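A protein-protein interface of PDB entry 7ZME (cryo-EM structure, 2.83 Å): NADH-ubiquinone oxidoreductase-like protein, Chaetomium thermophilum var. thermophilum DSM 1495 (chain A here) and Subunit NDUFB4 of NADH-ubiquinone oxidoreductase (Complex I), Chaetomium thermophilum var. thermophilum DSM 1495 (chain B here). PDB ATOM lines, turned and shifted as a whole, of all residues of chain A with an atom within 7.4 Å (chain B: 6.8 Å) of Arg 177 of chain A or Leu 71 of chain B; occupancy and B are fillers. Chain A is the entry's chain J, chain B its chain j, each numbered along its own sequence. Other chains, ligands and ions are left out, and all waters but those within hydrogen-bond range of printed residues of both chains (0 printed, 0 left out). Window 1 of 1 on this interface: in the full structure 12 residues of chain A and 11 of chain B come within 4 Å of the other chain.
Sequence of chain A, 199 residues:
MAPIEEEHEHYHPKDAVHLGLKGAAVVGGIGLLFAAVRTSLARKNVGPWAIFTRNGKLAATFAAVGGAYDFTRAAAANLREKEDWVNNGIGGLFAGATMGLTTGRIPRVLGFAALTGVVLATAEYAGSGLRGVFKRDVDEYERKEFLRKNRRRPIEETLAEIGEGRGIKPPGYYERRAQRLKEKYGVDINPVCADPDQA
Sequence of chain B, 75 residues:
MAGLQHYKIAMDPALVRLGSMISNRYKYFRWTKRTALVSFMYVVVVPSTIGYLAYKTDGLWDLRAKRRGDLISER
NZ of Lys 66 of chain B is in hydrogen-bond range of O of Asp 62 of chain B (2.9 Å).
NZ of Lys 66 of chain B lies within hydrogen-bond range of O of Leu 71 of chain B (2.4 Å).
The side-chain amino group (NZ) of Lys 66 of chain B lies within hydrogen-bond range of the backbone carbonyl oxygen (O) of Ile 72 of chain B, 3.4 Å away.
The side-chain amino group (NZ) of Lys 66 of chain B lies within salt-bridge range of the side-chain carboxylate (OE2) of Glu 74 of chain B (3.9 Å).
The side-chain hydroxyl (OG) of Ser 73 of chain B sits at hydrogen-bond distance from the chain-end carboxylate (O) of Arg 75 of chain B, 3.0 Å away.
Of the printed residues of chain B, Lys 169 of chain A touches Glu 74.
Arg 177 of chain A touches five residues of chain B.
Gly 186 of chain A touches none of the printed residues of chain B.
Of the printed residues of chain A, Asp 70 of chain B touches Arg 177 and Ile 189.
Of chain A, only Arg 177 (2.7 Å) and Tyr 185 (3.8 Å) come within 4 Å of Leu 71 of chain B.
Of the printed residues of chain A, Ser 73 of chain B touches Arg 177 (2.8 Å), Leu 181 (3.7 Å) and Tyr 185 (3.2 Å).
The nearest residue of chain A that does not touch Leu 71 of chain B is Ile 189 of chain A (4.2 Å).
OE2 of Glu 74 of chain B lies within salt-bridge range of NZ of Lys 169 of chain A (3.6 Å).
The side-chain hydroxyl (OH) of Tyr 173 of chain A lies within hydrogen-bond range of the side-chain carboxylate (OE1) of Glu 74 of chain B (3.1 Å).
The guanidinium group (NH2) of Arg 177 of chain A is in salt-bridge range of the side-chain carboxylate (OD1) of Asp 70 of chain B (2.6 Å).
The guanidinium group of Arg 177 of chain A sits at hydrogen-bond distance from the backbone carbonyl oxygen of Leu 71 of chain B (2.7 Å).
NH1 of Arg 177 of chain A is in hydrogen-bond range of O of Ser 73 of chain B, at 2.8 Å.
The backbone carbonyl oxygen (O) of Glu 74 of chain B lies within hydrogen-bond range of the guanidinium group (NH1) of Arg 180 of chain A (3.0 Å).
The side-chain hydroxyl (OH) of Tyr 185 of chain A sits at hydrogen-bond distance from the side-chain hydroxyl (OG) of Ser 73 of chain B, 3.2 Å away.
OH of Tyr 185 of chain A is in hydrogen-bond range of O of Arg 75 of chain B, 3.3 Å away.
The guanidinium group (NH1) of Arg 177 of chain A sits close to the side-chain amino group (NZ) of Lys 66 of chain B (3.1 Å).
Of the 20 printed residues of chain A, 8 touch a printed residue of chain B.
Hydrophobic or aromatic side chains of chain A within 4 Å of the printed part of chain B: Tyr 173, Leu 181, Tyr 185, Ile 189 and Pro 191.
Hydrophobic or aromatic side chains of chain B that line the printed part of chain A: Leu 71.
Among the printed residues, Asp or Glu carboxylates within 4 Å of a Lys or Arg side-chain nitrogen of the other chain: Lys 169 of chain A with Glu 74 of chain B (3.6 Å) and Arg 177 of chain A with Asp 70 of chain B (2.6 Å).
Among the printed residues, merely in contact across the chains: Arg 177 of chain A with Glu 74 of chain B, Leu 181 of chain A with Ser 73 of chain B, Tyr 185 of chain A with Leu 71 of chain B, Ile 189 of chain A with Gly 69 of chain B, Ile 189 of chain A with Asp 70 of chain B and Pro 191 of chain A with Arg 67 of chain B.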
ATOM      1  N   GLU A 164      14.746  20.665   6.739  1.00  0.00           N
ATOM      2  CA  GLU A 164      15.611  20.191   7.808  1.00  0.00           C
ATOM      3  C   GLU A 164      16.988  20.810   7.624  1.00  0.00           C
ATOM      4  O   GLU A 164      17.567  20.732   6.535  1.00  0.00           O
ATOM      5  CB  GLU A 164      15.695  18.667   7.799  1.00  0.00           C
ATOM      6  CG  GLU A 164      16.487  18.087   8.937  1.00  0.00           C
ATOM      7  CD  GLU A 164      16.453  16.575   8.951  1.00  0.00           C
ATOM      8  OE1 GLU A 164      15.864  15.983   8.022  1.00  0.00           O
ATOM      9  OE2 GLU A 164      17.005  15.976   9.897  1.00  0.00           O
ATOM     10  N   LYS A 169      17.673  20.896  13.478  1.00  0.00           N
ATOM     11  CA  LYS A 169      18.484  19.683  13.546  1.00  0.00           C
ATOM     12  C   LYS A 169      17.769  18.719  14.478  1.00  0.00           C
ATOM     13  O   LYS A 169      18.128  18.590  15.655  1.00  0.00           O
ATOM     14  CB  LYS A 169      19.894  20.004  14.038  1.00  0.00           C
ATOM     15  CG  LYS A 169      20.815  20.619  12.992  1.00  0.00           C
ATOM     16  CD  LYS A 169      22.273  20.354  13.325  1.00  0.00           C
ATOM     17  CE  LYS A 169      23.203  20.834  12.221  1.00  0.00           C
ATOM     18  NZ  LYS A 169      24.201  19.806  11.823  1.00  0.00           N
ATOM     19  N   GLY A 172      18.338  12.392  15.164  1.00  0.00           N
ATOM     20  CA  GLY A 172      18.578  11.602  13.976  1.00  0.00           C
ATOM     21  C   GLY A 172      19.000  12.393  12.760  1.00  0.00           C
ATOM     22  O   GLY A 172      19.068  11.825  11.665  1.00  0.00           O
ATOM     23  N   TYR A 173      19.280  13.689  12.917  1.00  0.00           N
ATOM     24  CA  TYR A 173      19.693  14.514  11.785  1.00  0.00           C
ATOM     25  C   TYR A 173      21.029  14.054  11.221  1.00  0.00           C
ATOM     26  O   TYR A 173      21.206  13.984  10.000  1.00  0.00           O
ATOM     27  CB  TYR A 173      19.775  15.981  12.211  1.00  0.00           C
ATOM     28  CG  TYR A 173      20.398  16.896  11.180  1.00  0.00           C
ATOM     29  CD1 TYR A 173      19.623  17.504  10.208  1.00  0.00           C
ATOM     30  CD2 TYR A 173      21.761  17.149  11.177  1.00  0.00           C
ATOM     31  CE1 TYR A 173      20.178  18.329   9.268  1.00  0.00           C
ATOM     32  CE2 TYR A 173      22.324  17.969  10.236  1.00  0.00           C
ATOM     33  CZ  TYR A 173      21.529  18.562   9.286  1.00  0.00           C
ATOM     34  OH  TYR A 173      22.093  19.393   8.344  1.00  0.00           O
ATOM     35  N   TYR A 174      21.988  13.748  12.095  1.00  0.00           N
ATOM     36  CA  TYR A 174      23.344  13.462  11.643  1.00  0.00           C
ATOM     37  C   TYR A 174      23.408  12.163  10.851  1.00  0.00           C
ATOM     38  O   TYR A 174      24.127  12.077   9.849  1.00  0.00           O
ATOM     39  CB  TYR A 174      24.289  13.413  12.842  1.00  0.00           C
ATOM     40  CG  TYR A 174      24.742  14.776  13.311  1.00  0.00           C
ATOM     41  CD1 TYR A 174      25.379  15.654  12.445  1.00  0.00           C
ATOM     42  CD2 TYR A 174      24.530  15.186  14.620  1.00  0.00           C
ATOM     43  CE1 TYR A 174      25.793  16.903  12.870  1.00  0.00           C
ATOM     44  CE2 TYR A 174      24.939  16.430  15.054  1.00  0.00           C
ATOM     45  CZ  TYR A 174      25.571  17.285  14.175  1.00  0.00           C
ATOM     46  OH  TYR A 174      25.981  18.527  14.607  1.00  0.00           O
ATOM     47  N   GLU A 175      22.675  11.139  11.291  1.00  0.00           N
ATOM     48  CA  GLU A 175      22.626   9.891  10.537  1.00  0.00           C
ATOM     49  C   GLU A 175      21.989  10.101   9.170  1.00  0.00           C
ATOM     50  O   GLU A 175      22.438   9.525   8.172  1.00  0.00           O
ATOM     51  CB  GLU A 175      21.866   8.828  11.329  1.00  0.00           C
ATOM     52  N   ARG A 176      20.937  10.919   9.106  1.00  0.00           N
ATOM     53  CA  ARG A 176      20.317  11.227   7.822  1.00  0.00           C
ATOM     54  C   ARG A 176      21.278  11.985   6.920  1.00  0.00           C
ATOM     55  O   ARG A 176      21.308  11.764   5.704  1.00  0.00           O
ATOM     56  CB  ARG A 176      19.040  12.038   8.036  1.00  0.00           C
ATOM     57  CG  ARG A 176      17.769  11.218   8.038  1.00  0.00           C
ATOM     58  CD  ARG A 176      16.598  12.063   8.492  1.00  0.00           C
ATOM     59  NE  ARG A 176      16.860  12.693   9.781  1.00  0.00           N
ATOM     60  CZ  ARG A 176      15.913  13.124  10.604  1.00  0.00           C
ATOM     61  NH1 ARG A 176      16.241  13.686  11.759  1.00  0.00           N
ATOM     62  NH2 ARG A 176      14.636  12.994  10.273  1.00  0.00           N
ATOM     63  N   ARG A 177      22.063  12.894   7.501  1.00  0.00           N
ATOM     64  CA  ARG A 177      23.043  13.641   6.724  1.00  0.00           C
ATOM     65  C   ARG A 177      24.093  12.721   6.121  1.00  0.00           C
ATOM     66  O   ARG A 177      24.515  12.917   4.976  1.00  0.00           O
ATOM     67  CB  ARG A 177      23.706  14.698   7.604  1.00  0.00           C
ATOM     68  CG  ARG A 177      24.719  15.544   6.874  1.00  0.00           C
ATOM     69  CD  ARG A 177      25.261  16.648   7.751  1.00  0.00           C
ATOM     70  NE  ARG A 177      26.306  17.396   7.064  1.00  0.00           N
ATOM     71  CZ  ARG A 177      27.601  17.105   7.137  1.00  0.00           C
ATOM     72  NH1 ARG A 177      28.486  17.837   6.474  1.00  0.00           N
ATOM     73  NH2 ARG A 177      28.010  16.079   7.869  1.00  0.00           N
ATOM     74  N   ALA A 178      24.531  11.713   6.878  1.00  0.00           N
ATOM     75  CA  ALA A 178      25.552  10.800   6.374  1.00  0.00           C
ATOM     76  C   ALA A 178      25.058  10.042   5.150  1.00  0.00           C
ATOM     77  O   ALA A 178      25.793   9.882   4.170  1.00  0.00           O
ATOM     78  CB  ALA A 178      25.977   9.830   7.474  1.00  0.00           C
ATOM     79  N   GLN A 179      23.814   9.563   5.191  1.00  0.00           N
ATOM     80  CA  GLN A 179      23.257   8.861   4.040  1.00  0.00           C
ATOM     81  C   GLN A 179      23.037   9.808   2.867  1.00  0.00           C
ATOM     82  O   GLN A 179      23.329   9.458   1.717  1.00  0.00           O
ATOM     83  CB  GLN A 179      21.949   8.174   4.427  1.00  0.00           C
ATOM     84  CG  GLN A 179      22.112   7.071   5.459  1.00  0.00           C
ATOM     85  CD  GLN A 179      20.817   6.326   5.723  1.00  0.00           C
ATOM     86  OE1 GLN A 179      19.938   6.261   4.863  1.00  0.00           O
ATOM     87  NE2 GLN A 179      20.694   5.757   6.917  1.00  0.00           N
ATOM     88  N   ARG A 180      22.519  11.009   3.136  1.00  0.00           N
ATOM     89  CA  ARG A 180      22.250  11.958   2.060  1.00  0.00           C
ATOM     90  C   ARG A 180      23.534  12.381   1.358  1.00  0.00           C
ATOM     91  O   ARG A 180      23.573  12.481   0.126  1.00  0.00           O
ATOM     92  CB  ARG A 180      21.510  13.176   2.609  1.00  0.00           C
ATOM     93  CG  ARG A 180      21.196  14.238   1.569  1.00  0.00           C
ATOM     94  CD  ARG A 180      20.323  15.349   2.140  1.00  0.00           C
ATOM     95  NE  ARG A 180      21.004  16.118   3.180  1.00  0.00           N
ATOM     96  CZ  ARG A 180      20.848  15.915   4.485  1.00  0.00           C
ATOM     97  NH1 ARG A 180      21.507  16.662   5.358  1.00  0.00           N
ATOM     98  NH2 ARG A 180      20.028  14.967   4.915  1.00  0.00           N
ATOM     99  N   LEU A 181      24.595  12.636   2.125  1.00  0.00           N
ATOM    100  CA  LEU A 181      25.875  12.986   1.518  1.00  0.00           C
ATOM    101  C   LEU A 181      26.449  11.828   0.713  1.00  0.00           C
ATOM    102  O   LEU A 181      27.101  12.050  -0.313  1.00  0.00           O
ATOM    103  CB  LEU A 181      26.869  13.423   2.592  1.00  0.00           C
ATOM    104  CG  LEU A 181      26.599  14.749   3.303  1.00  0.00           C
ATOM    105  CD1 LEU A 181      27.445  14.839   4.559  1.00  0.00           C
ATOM    106  CD2 LEU A 181      26.869  15.933   2.385  1.00  0.00           C
ATOM    107  N   LYS A 182      26.223  10.592   1.166  1.00  0.00           N
ATOM    108  CA  LYS A 182      26.787   9.432   0.482  1.00  0.00           C
ATOM    109  C   LYS A 182      26.238   9.296  -0.933  1.00  0.00           C
ATOM    110  O   LYS A 182      26.987   9.007  -1.872  1.00  0.00           O
ATOM    111  CB  LYS A 182      26.509   8.165   1.289  1.00  0.00           C
ATOM    112  CG  LYS A 182      27.074   6.897   0.674  1.00  0.00           C
ATOM    113  CD  LYS A 182      28.588   6.863   0.781  1.00  0.00           C
ATOM    114  CE  LYS A 182      29.147   5.551   0.257  1.00  0.00           C
ATOM    115  NZ  LYS A 182      28.757   4.401   1.117  1.00  0.00           N
ATOM    116  N   GLU A 183      24.932   9.497  -1.107  1.00  0.00           N
ATOM    117  CA  GLU A 183      24.332   9.319  -2.424  1.00  0.00           C
ATOM    118  C   GLU A 183      24.702  10.434  -3.392  1.00  0.00           C
ATOM    119  O   GLU A 183      24.746  10.195  -4.602  1.00  0.00           O
ATOM    120  CB  GLU A 183      22.812   9.218  -2.300  1.00  0.00           C
ATOM    121  CG  GLU A 183      22.335   7.955  -1.605  1.00  0.00           C
ATOM    122  CD  GLU A 183      20.826   7.815  -1.619  1.00  0.00           C
ATOM    123  OE1 GLU A 183      20.286   7.107  -0.743  1.00  0.00           O
ATOM    124  OE2 GLU A 183      20.181   8.413  -2.504  1.00  0.00           O
ATOM    125  N   TYR A 185      27.636  12.593  -3.057  1.00  0.00           N
ATOM    126  CA  TYR A 185      29.073  12.766  -3.210  1.00  0.00           C
ATOM    127  C   TYR A 185      29.867  11.470  -3.165  1.00  0.00           C
ATOM    128  O   TYR A 185      31.032  11.473  -3.577  1.00  0.00           O
ATOM    129  CB  TYR A 185      29.618  13.713  -2.128  1.00  0.00           C
ATOM    130  CG  TYR A 185      29.012  15.099  -2.165  1.00  0.00           C
ATOM    131  CD1 TYR A 185      28.571  15.653  -3.359  1.00  0.00           C
ATOM    132  CD2 TYR A 185      28.877  15.849  -1.005  1.00  0.00           C
ATOM    133  CE1 TYR A 185      28.014  16.916  -3.396  1.00  0.00           C
ATOM    134  CE2 TYR A 185      28.321  17.113  -1.034  1.00  0.00           C
ATOM    135  CZ  TYR A 185      27.892  17.641  -2.231  1.00  0.00           C
ATOM    136  OH  TYR A 185      27.339  18.900  -2.265  1.00  0.00           O
ATOM    137  N   GLY A 186      29.285  10.375  -2.688  1.00  0.00           N
ATOM    138  CA  GLY A 186      30.000   9.110  -2.628  1.00  0.00           C
ATOM    139  C   GLY A 186      31.185   9.099  -1.687  1.00  0.00           C
ATOM    140  O   GLY A 186      32.240   8.555  -2.034  1.00  0.00           O
ATOM    141  N   VAL A 187      31.039   9.687  -0.502  1.00  0.00           N
ATOM    142  CA  VAL A 187      32.106   9.745   0.490  1.00  0.00           C
ATOM    143  C   VAL A 187      31.559   9.246   1.819  1.00  0.00           C
ATOM    144  O   VAL A 187      30.498   9.696   2.266  1.00  0.00           O
ATOM    145  CB  VAL A 187      32.672  11.169   0.641  1.00  0.00           C
ATOM    146  CG1 VAL A 187      33.704  11.216   1.757  1.00  0.00           C
ATOM    147  CG2 VAL A 187      33.278  11.642  -0.671  1.00  0.00           C
ATOM    148  N   ASP A 188      32.278   8.319   2.445  1.00  0.00           N
ATOM    149  CA  ASP A 188      31.907   7.828   3.767  1.00  0.00           C
ATOM    150  C   ASP A 188      32.326   8.850   4.816  1.00  0.00           C
ATOM    151  O   ASP A 188      33.474   9.308   4.822  1.00  0.00           O
ATOM    152  CB  ASP A 188      32.557   6.474   4.037  1.00  0.00           C
ATOM    153  N   ILE A 189      31.402   9.209   5.701  1.00  0.00           N
ATOM    154  CA  ILE A 189      31.658  10.242   6.698  1.00  0.00           C
ATOM    155  C   ILE A 189      32.276   9.596   7.933  1.00  0.00           C
ATOM    156  O   ILE A 189      31.697   8.679   8.523  1.00  0.00           O
ATOM    157  CB  ILE A 189      30.371  10.997   7.055  1.00  0.00           C
ATOM    158  CG1 ILE A 189      29.948  11.898   5.892  1.00  0.00           C
ATOM    159  CG2 ILE A 189      30.557  11.804   8.330  1.00  0.00           C
ATOM    160  CD1 ILE A 189      30.694  13.210   5.827  1.00  0.00           C
ATOM    161  N   PRO A 191      34.696  11.524  10.895  1.00  0.00           N
ATOM    162  CA  PRO A 191      35.609  12.505  11.495  1.00  0.00           C
ATOM    163  C   PRO A 191      36.723  11.838  12.290  1.00  0.00           C
ATOM    164  O   PRO A 191      36.552  10.756  12.857  1.00  0.00           O
ATOM    165  CB  PRO A 191      34.698  13.330  12.412  1.00  0.00           C
ATOM    166  CG  PRO A 191      33.287  12.954  12.066  1.00  0.00           C
ATOM    167  CD  PRO A 191      33.298  11.980  10.937  1.00  0.00           C
ATOM    168  N   ASP B  62      28.035  24.504   6.444  1.00  0.00           N
ATOM    169  CA  ASP B  62      28.133  24.681   7.885  1.00  0.00           C
ATOM    170  C   ASP B  62      29.536  24.298   8.321  1.00  0.00           C
ATOM    171  O   ASP B  62      30.045  23.246   7.929  1.00  0.00           O
ATOM    172  CB  ASP B  62      27.095  23.839   8.624  1.00  0.00           C
ATOM    173  CG  ASP B  62      27.093  24.091  10.115  1.00  0.00           C
ATOM    174  OD1 ASP B  62      27.358  25.242  10.519  1.00  0.00           O
ATOM    175  OD2 ASP B  62      26.822  23.145  10.883  1.00  0.00           O
ATOM    176  N   LEU B  63      30.156  25.159   9.119  1.00  0.00           N
ATOM    177  CA  LEU B  63      31.535  24.978   9.541  1.00  0.00           C
ATOM    178  C   LEU B  63      31.656  24.462  10.963  1.00  0.00           C
ATOM    179  O   LEU B  63      32.757  24.087  11.368  1.00  0.00           O
ATOM    180  CB  LEU B  63      32.291  26.307   9.430  1.00  0.00           C
ATOM    181  CG  LEU B  63      33.183  26.573   8.224  1.00  0.00           C
ATOM    182  CD1 LEU B  63      32.402  26.379   6.944  1.00  0.00           C
ATOM    183  CD2 LEU B  63      33.717  27.980   8.291  1.00  0.00           C
ATOM    184  N   LYS B  66      33.415  20.924  12.002  1.00  0.00           N
ATOM    185  CA  LYS B  66      33.753  19.957  10.966  1.00  0.00           C
ATOM    186  C   LYS B  66      35.200  19.502  11.112  1.00  0.00           C
ATOM    187  O   LYS B  66      36.129  20.306  10.995  1.00  0.00           O
ATOM    188  CB  LYS B  66      33.519  20.556   9.583  1.00  0.00           C
ATOM    189  CG  LYS B  66      32.112  21.059   9.357  1.00  0.00           C
ATOM    190  CD  LYS B  66      31.092  19.994   9.688  1.00  0.00           C
ATOM    191  CE  LYS B  66      29.702  20.417   9.267  1.00  0.00           C
ATOM    192  NZ  LYS B  66      29.544  20.397   7.793  1.00  0.00           N
ATOM    193  N   ARG B  67      35.387  18.211  11.360  1.00  0.00           N
ATOM    194  CA  ARG B  67      36.710  17.626  11.474  1.00  0.00           C
ATOM    195  C   ARG B  67      37.190  17.175  10.098  1.00  0.00           C
ATOM    196  O   ARG B  67      36.551  17.421   9.074  1.00  0.00           O
ATOM    197  CB  ARG B  67      36.698  16.439  12.431  1.00  0.00           C
ATOM    198  CG  ARG B  67      36.437  16.753  13.887  1.00  0.00           C
ATOM    199  CD  ARG B  67      36.471  15.446  14.663  1.00  0.00           C
ATOM    200  NE  ARG B  67      36.248  15.599  16.093  1.00  0.00           N
ATOM    201  CZ  ARG B  67      35.048  15.542  16.657  1.00  0.00           C
ATOM    202  NH1 ARG B  67      33.976  15.330  15.908  1.00  0.00           N
ATOM    203  NH2 ARG B  67      34.918  15.682  17.968  1.00  0.00           N
ATOM    204  N   GLY B  69      37.218  14.331   7.676  1.00  0.00           N
ATOM    205  CA  GLY B  69      36.301  13.224   7.513  1.00  0.00           C
ATOM    206  C   GLY B  69      34.862  13.648   7.334  1.00  0.00           C
ATOM    207  O   GLY B  69      34.051  12.846   6.853  1.00  0.00           O
ATOM    208  N   ASP B  70      34.518  14.873   7.710  1.00  0.00           N
ATOM    209  CA  ASP B  70      33.230  15.471   7.407  1.00  0.00           C
ATOM    210  C   ASP B  70      33.387  16.399   6.207  1.00  0.00           C
ATOM    211  O   ASP B  70      34.461  16.507   5.608  1.00  0.00           O
ATOM    212  CB  ASP B  70      32.682  16.216   8.624  1.00  0.00           C
ATOM    213  CG  ASP B  70      31.171  16.356   8.592  1.00  0.00           C
ATOM    214  OD1 ASP B  70      30.570  16.064   7.537  1.00  0.00           O
ATOM    215  OD2 ASP B  70      30.588  16.759   9.619  1.00  0.00           O
ATOM    216  N   LEU B  71      32.302  17.075   5.854  1.00  0.00           N
ATOM    217  CA  LEU B  71      32.298  18.001   4.737  1.00  0.00           C
ATOM    218  C   LEU B  71      31.621  19.298   5.148  1.00  0.00           C
ATOM    219  O   LEU B  71      30.730  19.308   6.000  1.00  0.00           O
ATOM    220  CB  LEU B  71      31.585  17.407   3.521  1.00  0.00           C
ATOM    221  CG  LEU B  71      32.233  16.164   2.916  1.00  0.00           C
ATOM    222  CD1 LEU B  71      31.348  15.576   1.831  1.00  0.00           C
ATOM    223  CD2 LEU B  71      33.608  16.503   2.368  1.00  0.00           C
ATOM    224  N   ILE B  72      32.065  20.398   4.540  1.00  0.00           N
ATOM    225  CA  ILE B  72      31.399  21.678   4.752  1.00  0.00           C
ATOM    226  C   ILE B  72      29.957  21.604   4.275  1.00  0.00           C
ATOM    227  O   ILE B  72      29.042  22.127   4.922  1.00  0.00           O
ATOM    228  CB  ILE B  72      32.167  22.804   4.038  1.00  0.00           C
ATOM    229  CG1 ILE B  72      33.617  22.856   4.520  1.00  0.00           C
ATOM    230  CG2 ILE B  72      31.480  24.135   4.257  1.00  0.00           C
ATOM    231  CD1 ILE B  72      34.429  23.927   3.851  1.00  0.00           C
ATOM    232  N   SER B  73      29.734  20.951   3.140  1.00  0.00           N
ATOM    233  CA  SER B  73      28.399  20.853   2.574  1.00  0.00           C
ATOM    234  C   SER B  73      27.494  20.009   3.457  1.00  0.00           C
ATOM    235  O   SER B  73      27.921  19.012   4.044  1.00  0.00           O
ATOM    236  CB  SER B  73      28.466  20.255   1.171  1.00  0.00           C
ATOM    237  OG  SER B  73      27.279  20.514   0.449  1.00  0.00           O
ATOM    238  N   GLU B  74      26.237  20.431   3.564  1.00  0.00           N
ATOM    239  CA  GLU B  74      25.201  19.641   4.205  1.00  0.00           C
ATOM    240  C   GLU B  74      24.032  19.345   3.284  1.00  0.00           C
ATOM    241  O   GLU B  74      23.202  18.493   3.615  1.00  0.00           O
ATOM    242  CB  GLU B  74      24.684  20.340   5.467  1.00  0.00           C
ATOM    243  CG  GLU B  74      25.699  20.421   6.580  1.00  0.00           C
ATOM    244  CD  GLU B  74      25.167  21.122   7.801  1.00  0.00           C
ATOM    245  OE1 GLU B  74      24.043  21.663   7.733  1.00  0.00           O
ATOM    246  OE2 GLU B  74      25.843  21.072   8.850  1.00  0.00           O
ATOM    247  N   ARG B  75      23.943  20.020   2.144  1.00  0.00           N
ATOM    248  CA  ARG B  75      22.882  19.777   1.180  1.00  0.00           C
ATOM    249  C   ARG B  75      23.457  19.140  -0.080  1.00  0.00           C
ATOM    250  O   ARG B  75      24.621  19.363  -0.411  1.00  0.00           O
ATOM    251  CB  ARG B  75      22.161  21.084   0.846  1.00  0.00           C
ATOM    252  CG  ARG B  75      21.052  20.946  -0.180  1.00  0.00           C
ATOM    253  CD  ARG B  75      19.985  22.005   0.022  1.00  0.00           C
ATOM    254  NE  ARG B  75      20.535  23.309   0.388  1.00  0.00           N
ATOM    255  CZ  ARG B  75      21.134  24.141  -0.460  1.00  0.00           C
ATOM    256  NH1 ARG B  75      21.594  25.304  -0.031  1.00  0.00           N
ATOM    257  NH2 ARG B  75      21.254  23.822  -1.742  1.00  0.00           N
ATOM    258  OXT ARG B  75      22.786  18.391  -0.791  1.00  0.00           O
